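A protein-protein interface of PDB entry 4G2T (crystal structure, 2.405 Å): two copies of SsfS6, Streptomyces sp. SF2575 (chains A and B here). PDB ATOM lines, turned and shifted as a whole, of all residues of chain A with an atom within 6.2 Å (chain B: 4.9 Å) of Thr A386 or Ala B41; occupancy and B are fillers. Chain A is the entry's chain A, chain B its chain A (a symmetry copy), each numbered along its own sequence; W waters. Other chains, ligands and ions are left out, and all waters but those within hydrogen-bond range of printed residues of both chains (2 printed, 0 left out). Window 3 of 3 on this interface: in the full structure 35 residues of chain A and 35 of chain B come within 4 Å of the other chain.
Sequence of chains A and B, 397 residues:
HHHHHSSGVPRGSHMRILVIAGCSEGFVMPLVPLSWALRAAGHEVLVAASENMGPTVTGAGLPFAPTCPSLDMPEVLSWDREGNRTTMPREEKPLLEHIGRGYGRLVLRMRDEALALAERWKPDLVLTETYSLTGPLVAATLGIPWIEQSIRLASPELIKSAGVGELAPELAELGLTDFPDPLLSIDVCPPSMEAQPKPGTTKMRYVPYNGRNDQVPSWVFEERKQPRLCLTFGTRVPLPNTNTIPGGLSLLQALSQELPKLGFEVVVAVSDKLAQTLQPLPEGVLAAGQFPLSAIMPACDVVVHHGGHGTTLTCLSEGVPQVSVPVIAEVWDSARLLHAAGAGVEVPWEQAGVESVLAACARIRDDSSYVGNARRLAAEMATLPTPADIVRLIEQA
The guanidinium group (NH1) of Arg A205 is in hydrogen-bond range of the backbone carbonyl oxygen (O) of Gly B42. O of Ala B40 is in hydrogen-bond range of N of Ala A388 (3.3 Å).
N of Arg A205 sits at hydrogen-bond distance from O of Pro A385 (2.5 Å). The backbone NH (N) of Ala A388 lies close to the side-chain hydroxyl (OG1) of Thr A386 (3.2 Å). The backbone NH of Thr A386 lies within hydrogen-bond range of the side-chain carboxylate of Asp A389, 2.7 Å away. O of Ala A388 sits at hydrogen-bond distance from NE of Arg A392 (3.4 Å). NH1 of Arg B39 sits at hydrogen-bond distance from O of His B43.
CG1 of Val A207 touches NE of Arg B39, 3.4 Å away. Thr A386 touches Ala B40 (CB to O, 3.5 Å). Thr A386 touches Ala B41 (CG2 to O, 3.4 Å). CD of Pro A387 touches O of Ala B40 (3.3 Å).
Printed residues of chain B within 4 Å of Arg A205: Gly B42 (3.1 Å). Thr A386 touches two residues of chain B. Of the printed residues of chain B, Pro A387 touches Ala B40. Asp A389 touches none of the printed residues of chain B. Leu B38 touches none of the printed residues of chain A. Printed residues of chain A within 4 Å of Arg B39: Val A207. Printed residues of chain A within 4 Å of Ala B40: Thr A386 (3.5 Å), Pro A387 (3.3 Å) and Ala A388 (3.3 Å). The nearest residue of chain B that does not touch Thr A386 is Gly B42 (4.3 Å).
Of the 15 printed residues of chain A, 5 touch a printed residue of chain B. Hydrophobic or aromatic side chains of chain A within 4 Å of the printed part of chain B: Val A207, Pro A387 and Ala A388. Along chain A the printed residues that touch a printed residue of chain B span positions 205 to 388. Of the 9 printed residues of chain B, 4 touch a printed residue of chain A. Among the printed residues, 6 pairs touch across the chains. Among the printed residues, no Asp or Glu carboxylate lies within 4 Å of a Lys or Arg side-chain nitrogen of the other chain.
Position printed for both chains: 391.
Water W2 bridges OE2 of Glu B395 (2.5 Å) and NH2 of Arg A392 (3.2 Å). Water W1 lies within hydrogen-bond range of the backbone carbonyl oxygen (O) of Gly B42, the guanidinium group (NH1) of Arg B39 and the guanidinium group (NH2) of Arg A205.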
ATOM      1  N   LEU A  34     -29.104  26.075  14.454  1.00  0.00           N
ATOM      2  CA  LEU A  34     -28.218  26.773  13.529  1.00  0.00           C
ATOM      3  C   LEU A  34     -28.409  28.283  13.628  1.00  0.00           C
ATOM      4  O   LEU A  34     -27.466  29.050  13.436  1.00  0.00           O
ATOM      5  CB  LEU A  34     -28.442  26.298  12.091  1.00  0.00           C
ATOM      6  CG  LEU A  34     -27.450  26.836  11.056  1.00  0.00           C
ATOM      7  CD1 LEU A  34     -26.023  26.480  11.448  1.00  0.00           C
ATOM      8  CD2 LEU A  34     -27.770  26.313   9.666  1.00  0.00           C
ATOM      9  N   LYS A 203     -22.188  17.723   5.536  1.00  0.00           N
ATOM     10  CA  LYS A 203     -22.828  17.035   6.652  1.00  0.00           C
ATOM     11  C   LYS A 203     -22.774  17.860   7.932  1.00  0.00           C
ATOM     12  O   LYS A 203     -21.773  18.515   8.221  1.00  0.00           O
ATOM     13  CB  LYS A 203     -22.188  15.664   6.883  1.00  0.00           C
ATOM     14  CG  LYS A 203     -22.499  14.643   5.801  1.00  0.00           C
ATOM     15  CD  LYS A 203     -23.999  14.488   5.611  1.00  0.00           C
ATOM     16  CE  LYS A 203     -24.321  13.399   4.600  1.00  0.00           C
ATOM     17  NZ  LYS A 203     -23.895  12.056   5.081  1.00  0.00           N
ATOM     18  N   MET A 204     -23.864  17.826   8.694  1.00  0.00           N
ATOM     19  CA  MET A 204     -23.924  18.509   9.979  1.00  0.00           C
ATOM     20  C   MET A 204     -24.566  17.609  11.030  1.00  0.00           C
ATOM     21  O   MET A 204     -25.541  16.911  10.747  1.00  0.00           O
ATOM     22  CB  MET A 204     -24.712  19.816   9.868  1.00  0.00           C
ATOM     23  CG  MET A 204     -24.726  20.635  11.154  1.00  0.00           C
ATOM     24  SD  MET A 204     -26.274  21.813  11.337  1.00  0.00           S
ATOM     25  CE  MET A 204     -25.886  23.092   9.933  1.00  0.00           C
ATOM     26  N   ARG A 205     -24.013  17.624  12.239  1.00  0.00           N
ATOM     27  CA  ARG A 205     -24.594  16.880  13.347  1.00  0.00           C
ATOM     28  C   ARG A 205     -25.953  17.463  13.710  1.00  0.00           C
ATOM     29  O   ARG A 205     -26.112  18.682  13.790  1.00  0.00           O
ATOM     30  CB  ARG A 205     -23.674  16.919  14.569  1.00  0.00           C
ATOM     31  CG  ARG A 205     -24.271  16.258  15.802  1.00  0.00           C
ATOM     32  CD  ARG A 205     -23.373  16.412  17.017  1.00  0.00           C
ATOM     33  NE  ARG A 205     -23.940  15.753  18.189  1.00  0.00           N
ATOM     34  CZ  ARG A 205     -23.406  15.801  19.406  1.00  0.00           C
ATOM     35  NH1 ARG A 205     -22.289  16.482  19.616  1.00  0.00           N
ATOM     36  NH2 ARG A 205     -23.993  15.169  20.414  1.00  0.00           N
ATOM     37  N   VAL A 207     -28.274  18.581  16.156  1.00  0.00           N
ATOM     38  CA  VAL A 207     -28.518  18.992  17.531  1.00  0.00           C
ATOM     39  C   VAL A 207     -30.010  19.243  17.690  1.00  0.00           C
ATOM     40  O   VAL A 207     -30.559  20.157  17.078  1.00  0.00           O
ATOM     41  CB  VAL A 207     -27.734  20.265  17.889  1.00  0.00           C
ATOM     42  CG1 VAL A 207     -28.099  20.735  19.288  1.00  0.00           C
ATOM     43  CG2 VAL A 207     -26.238  20.013  17.778  1.00  0.00           C
ATOM     44  N   ALA A 382     -22.420  12.195  16.040  1.00  0.00           N
ATOM     45  CA  ALA A 382     -21.590  13.012  16.919  1.00  0.00           C
ATOM     46  C   ALA A 382     -20.262  13.394  16.265  1.00  0.00           C
ATOM     47  O   ALA A 382     -19.637  14.384  16.643  1.00  0.00           O
ATOM     48  CB  ALA A 382     -21.347  12.292  18.238  1.00  0.00           C
ATOM     49  N   LEU A 384     -19.992  14.126  13.048  1.00  0.00           N
ATOM     50  CA  LEU A 384     -20.306  15.122  12.031  1.00  0.00           C
ATOM     51  C   LEU A 384     -20.097  16.543  12.552  1.00  0.00           C
ATOM     52  O   LEU A 384     -20.196  16.783  13.756  1.00  0.00           O
ATOM     53  CB  LEU A 384     -21.748  14.942  11.546  1.00  0.00           C
ATOM     54  CG  LEU A 384     -22.079  13.584  10.927  1.00  0.00           C
ATOM     55  CD1 LEU A 384     -23.535  13.536  10.492  1.00  0.00           C
ATOM     56  CD2 LEU A 384     -21.154  13.286   9.755  1.00  0.00           C
ATOM     57  N   PRO A 385     -19.793  17.486  11.644  1.00  0.00           N
ATOM     58  CA  PRO A 385     -19.614  18.896  12.007  1.00  0.00           C
ATOM     59  C   PRO A 385     -20.822  19.458  12.751  1.00  0.00           C
ATOM     60  O   PRO A 385     -21.961  19.118  12.432  1.00  0.00           O
ATOM     61  CB  PRO A 385     -19.468  19.585  10.649  1.00  0.00           C
ATOM     62  CG  PRO A 385     -18.882  18.541   9.772  1.00  0.00           C
ATOM     63  CD  PRO A 385     -19.499  17.247  10.219  1.00  0.00           C
ATOM     64  N   THR A 386     -20.562  20.304  13.741  1.00  0.00           N
ATOM     65  CA  THR A 386     -21.622  20.920  14.525  1.00  0.00           C
ATOM     66  C   THR A 386     -22.192  22.114  13.767  1.00  0.00           C
ATOM     67  O   THR A 386     -21.567  22.601  12.824  1.00  0.00           O
ATOM     68  CB  THR A 386     -21.086  21.396  15.891  1.00  0.00           C
ATOM     69  OG1 THR A 386     -20.193  22.500  15.699  1.00  0.00           O
ATOM     70  CG2 THR A 386     -20.354  20.268  16.599  1.00  0.00           C
ATOM     71  N   PRO A 387     -23.388  22.583  14.163  1.00  0.00           N
ATOM     72  CA  PRO A 387     -23.910  23.834  13.603  1.00  0.00           C
ATOM     73  C   PRO A 387     -22.926  24.983  13.802  1.00  0.00           C
ATOM     74  O   PRO A 387     -22.882  25.903  12.987  1.00  0.00           O
ATOM     75  CB  PRO A 387     -25.176  24.075  14.424  1.00  0.00           C
ATOM     76  CG  PRO A 387     -25.636  22.712  14.793  1.00  0.00           C
ATOM     77  CD  PRO A 387     -24.387  21.899  15.007  1.00  0.00           C
ATOM     78  N   ALA A 388     -22.146  24.920  14.877  1.00  0.00           N
ATOM     79  CA  ALA A 388     -21.106  25.908  15.131  1.00  0.00           C
ATOM     80  C   ALA A 388     -20.005  25.810  14.079  1.00  0.00           C
ATOM     81  O   ALA A 388     -19.485  26.827  13.619  1.00  0.00           O
ATOM     82  CB  ALA A 388     -20.529  25.723  16.527  1.00  0.00           C
ATOM     83  N   ASP A 389     -19.657  24.582  13.704  1.00  0.00           N
ATOM     84  CA  ASP A 389     -18.656  24.350  12.667  1.00  0.00           C
ATOM     85  C   ASP A 389     -19.143  24.878  11.322  1.00  0.00           C
ATOM     86  O   ASP A 389     -18.365  25.413  10.533  1.00  0.00           O
ATOM     87  CB  ASP A 389     -18.338  22.857  12.548  1.00  0.00           C
ATOM     88  CG  ASP A 389     -17.766  22.273  13.826  1.00  0.00           C
ATOM     89  OD1 ASP A 389     -17.082  23.009  14.565  1.00  0.00           O
ATOM     90  OD2 ASP A 389     -18.000  21.074  14.089  1.00  0.00           O
ATOM     91  N   ILE A 390     -20.439  24.724  11.072  1.00  0.00           N
ATOM     92  CA  ILE A 390     -21.041  25.136   9.809  1.00  0.00           C
ATOM     93  C   ILE A 390     -21.087  26.657   9.667  1.00  0.00           C
ATOM     94  O   ILE A 390     -20.914  27.191   8.570  1.00  0.00           O
ATOM     95  CB  ILE A 390     -22.453  24.534   9.648  1.00  0.00           C
ATOM     96  CG1 ILE A 390     -22.365  23.006   9.610  1.00  0.00           C
ATOM     97  CG2 ILE A 390     -23.132  25.053   8.390  1.00  0.00           C
ATOM     98  CD1 ILE A 390     -21.552  22.469   8.453  1.00  0.00           C
ATOM     99  N   VAL A 391     -21.311  27.348  10.781  1.00  0.00           N
ATOM    100  CA  VAL A 391     -21.319  28.809  10.795  1.00  0.00           C
ATOM    101  C   VAL A 391     -20.006  29.369  10.253  1.00  0.00           C
ATOM    102  O   VAL A 391     -20.000  30.320   9.471  1.00  0.00           O
ATOM    103  CB  VAL A 391     -21.575  29.363  12.214  1.00  0.00           C
ATOM    104  CG1 VAL A 391     -21.276  30.853  12.275  1.00  0.00           C
ATOM    105  CG2 VAL A 391     -23.007  29.089  12.639  1.00  0.00           C
ATOM    106  N   ARG A 392     -18.898  28.759  10.665  1.00  0.00           N
ATOM    107  CA  ARG A 392     -17.577  29.156  10.192  1.00  0.00           C
ATOM    108  C   ARG A 392     -17.465  28.977   8.682  1.00  0.00           C
ATOM    109  O   ARG A 392     -16.969  29.859   7.982  1.00  0.00           O
ATOM    110  CB  ARG A 392     -16.492  28.344  10.899  1.00  0.00           C
ATOM    111  CG  ARG A 392     -16.557  28.428  12.413  1.00  0.00           C
ATOM    112  CD  ARG A 392     -15.716  27.344  13.059  1.00  0.00           C
ATOM    113  NE  ARG A 392     -16.154  27.063  14.422  1.00  0.00           N
ATOM    114  CZ  ARG A 392     -16.074  25.868  14.999  1.00  0.00           C
ATOM    115  NH1 ARG A 392     -15.572  24.839  14.329  1.00  0.00           N
ATOM    116  NH2 ARG A 392     -16.500  25.699  16.243  1.00  0.00           N
ATOM    117  N   ALA B  37     -24.195  28.912  22.742  1.00  0.00           N
ATOM    118  CA  ALA B  37     -22.954  28.721  22.000  1.00  0.00           C
ATOM    119  C   ALA B  37     -22.385  27.334  22.285  1.00  0.00           C
ATOM    120  O   ALA B  37     -21.806  26.698  21.408  1.00  0.00           O
ATOM    121  CB  ALA B  37     -21.948  29.800  22.358  1.00  0.00           C
ATOM    122  N   LEU B  38     -22.560  26.874  23.521  1.00  0.00           N
ATOM    123  CA  LEU B  38     -22.145  25.529  23.904  1.00  0.00           C
ATOM    124  C   LEU B  38     -23.057  24.486  23.271  1.00  0.00           C
ATOM    125  O   LEU B  38     -22.591  23.465  22.766  1.00  0.00           O
ATOM    126  CB  LEU B  38     -22.157  25.377  25.425  1.00  0.00           C
ATOM    127  CG  LEU B  38     -21.054  26.106  26.191  1.00  0.00           C
ATOM    128  CD1 LEU B  38     -21.336  26.085  27.685  1.00  0.00           C
ATOM    129  CD2 LEU B  38     -19.698  25.485  25.895  1.00  0.00           C
ATOM    130  N   ARG B  39     -24.359  24.751  23.303  1.00  0.00           N
ATOM    131  CA  ARG B  39     -25.344  23.843  22.726  1.00  0.00           C
ATOM    132  C   ARG B  39     -25.163  23.737  21.216  1.00  0.00           C
ATOM    133  O   ARG B  39     -25.389  22.682  20.625  1.00  0.00           O
ATOM    134  CB  ARG B  39     -26.764  24.306  23.062  1.00  0.00           C
ATOM    135  CG  ARG B  39     -27.857  23.369  22.575  1.00  0.00           C
ATOM    136  CD  ARG B  39     -27.632  21.957  23.087  1.00  0.00           C
ATOM    137  NE  ARG B  39     -28.633  21.018  22.593  1.00  0.00           N
ATOM    138  CZ  ARG B  39     -28.590  19.705  22.798  1.00  0.00           C
ATOM    139  NH1 ARG B  39     -27.591  19.173  23.486  1.00  0.00           N
ATOM    140  NH2 ARG B  39     -29.545  18.925  22.311  1.00  0.00           N
ATOM    141  N   ALA B  40     -24.745  24.839  20.600  1.00  0.00           N
ATOM    142  CA  ALA B  40     -24.498  24.867  19.164  1.00  0.00           C
ATOM    143  C   ALA B  40     -23.298  24.002  18.796  1.00  0.00           C
ATOM    144  O   ALA B  40     -23.198  23.508  17.673  1.00  0.00           O
ATOM    145  CB  ALA B  40     -24.286  26.297  18.693  1.00  0.00           C
ATOM    146  N   ALA B  41     -22.389  23.823  19.748  1.00  0.00           N
ATOM    147  CA  ALA B  41     -21.196  23.015  19.524  1.00  0.00           C
ATOM    148  C   ALA B  41     -21.435  21.549  19.877  1.00  0.00           C
ATOM    149  O   ALA B  41     -20.492  20.766  19.982  1.00  0.00           O
ATOM    150  CB  ALA B  41     -20.017  23.571  20.310  1.00  0.00           C
ATOM    151  N   GLY B  42     -22.701  21.189  20.065  1.00  0.00           N
ATOM    152  CA  GLY B  42     -23.081  19.804  20.285  1.00  0.00           C
ATOM    153  C   GLY B  42     -23.034  19.349  21.729  1.00  0.00           C
ATOM    154  O   GLY B  42     -23.178  18.160  22.015  1.00  0.00           O
ATOM    155  N   HIS B  43     -22.839  20.289  22.647  1.00  0.00           N
ATOM    156  CA  HIS B  43     -22.741  19.957  24.064  1.00  0.00           C
ATOM    157  C   HIS B  43     -24.104  19.958  24.746  1.00  0.00           C
ATOM    158  O   HIS B  43     -25.058  20.556  24.253  1.00  0.00           O
ATOM    159  CB  HIS B  43     -21.797  20.926  24.777  1.00  0.00           C
ATOM    160  CG  HIS B  43     -20.445  21.023  24.141  1.00  0.00           C
ATOM    161  ND1 HIS B  43     -19.483  20.047  24.282  1.00  0.00           N
ATOM    162  CD2 HIS B  43     -19.896  21.980  23.355  1.00  0.00           C
ATOM    163  CE1 HIS B  43     -18.400  20.399  23.612  1.00  0.00           C
ATOM    164  NE2 HIS B  43     -18.626  21.569  23.040  1.00  0.00           N
ATOM    165  N   VAL B 391     -16.121  29.025  23.243  1.00  0.00           N
ATOM    166  CA  VAL B 391     -16.464  27.611  23.369  1.00  0.00           C
ATOM    167  C   VAL B 391     -15.303  26.724  22.924  1.00  0.00           C
ATOM    168  O   VAL B 391     -14.982  25.730  23.576  1.00  0.00           O
ATOM    169  CB  VAL B 391     -17.729  27.258  22.557  1.00  0.00           C
ATOM    170  CG1 VAL B 391     -17.897  25.751  22.443  1.00  0.00           C
ATOM    171  CG2 VAL B 391     -18.959  27.883  23.194  1.00  0.00           C
ATOM    172  N   GLU B 395     -13.191  24.043  24.987  1.00  0.00           N
ATOM    173  CA  GLU B 395     -13.005  22.683  24.493  1.00  0.00           C
ATOM    174  C   GLU B 395     -11.527  22.338  24.360  1.00  0.00           C
ATOM    175  O   GLU B 395     -11.122  21.197  24.581  1.00  0.00           O
ATOM    176  CB  GLU B 395     -13.681  22.515  23.131  1.00  0.00           C
ATOM    177  CG  GLU B 395     -15.198  22.544  23.162  1.00  0.00           C
ATOM    178  CD  GLU B 395     -15.802  22.575  21.769  1.00  0.00           C
ATOM    179  OE1 GLU B 395     -16.747  21.801  21.511  1.00  0.00           O
ATOM    180  OE2 GLU B 395     -15.332  23.376  20.934  1.00  0.00           O
HETATM  181  O   HOH W   1     -25.846  16.640  22.644  1.00  0.00           O
HETATM  182  O   HOH W   2     -16.699  24.402  19.168  1.00  0.00           O
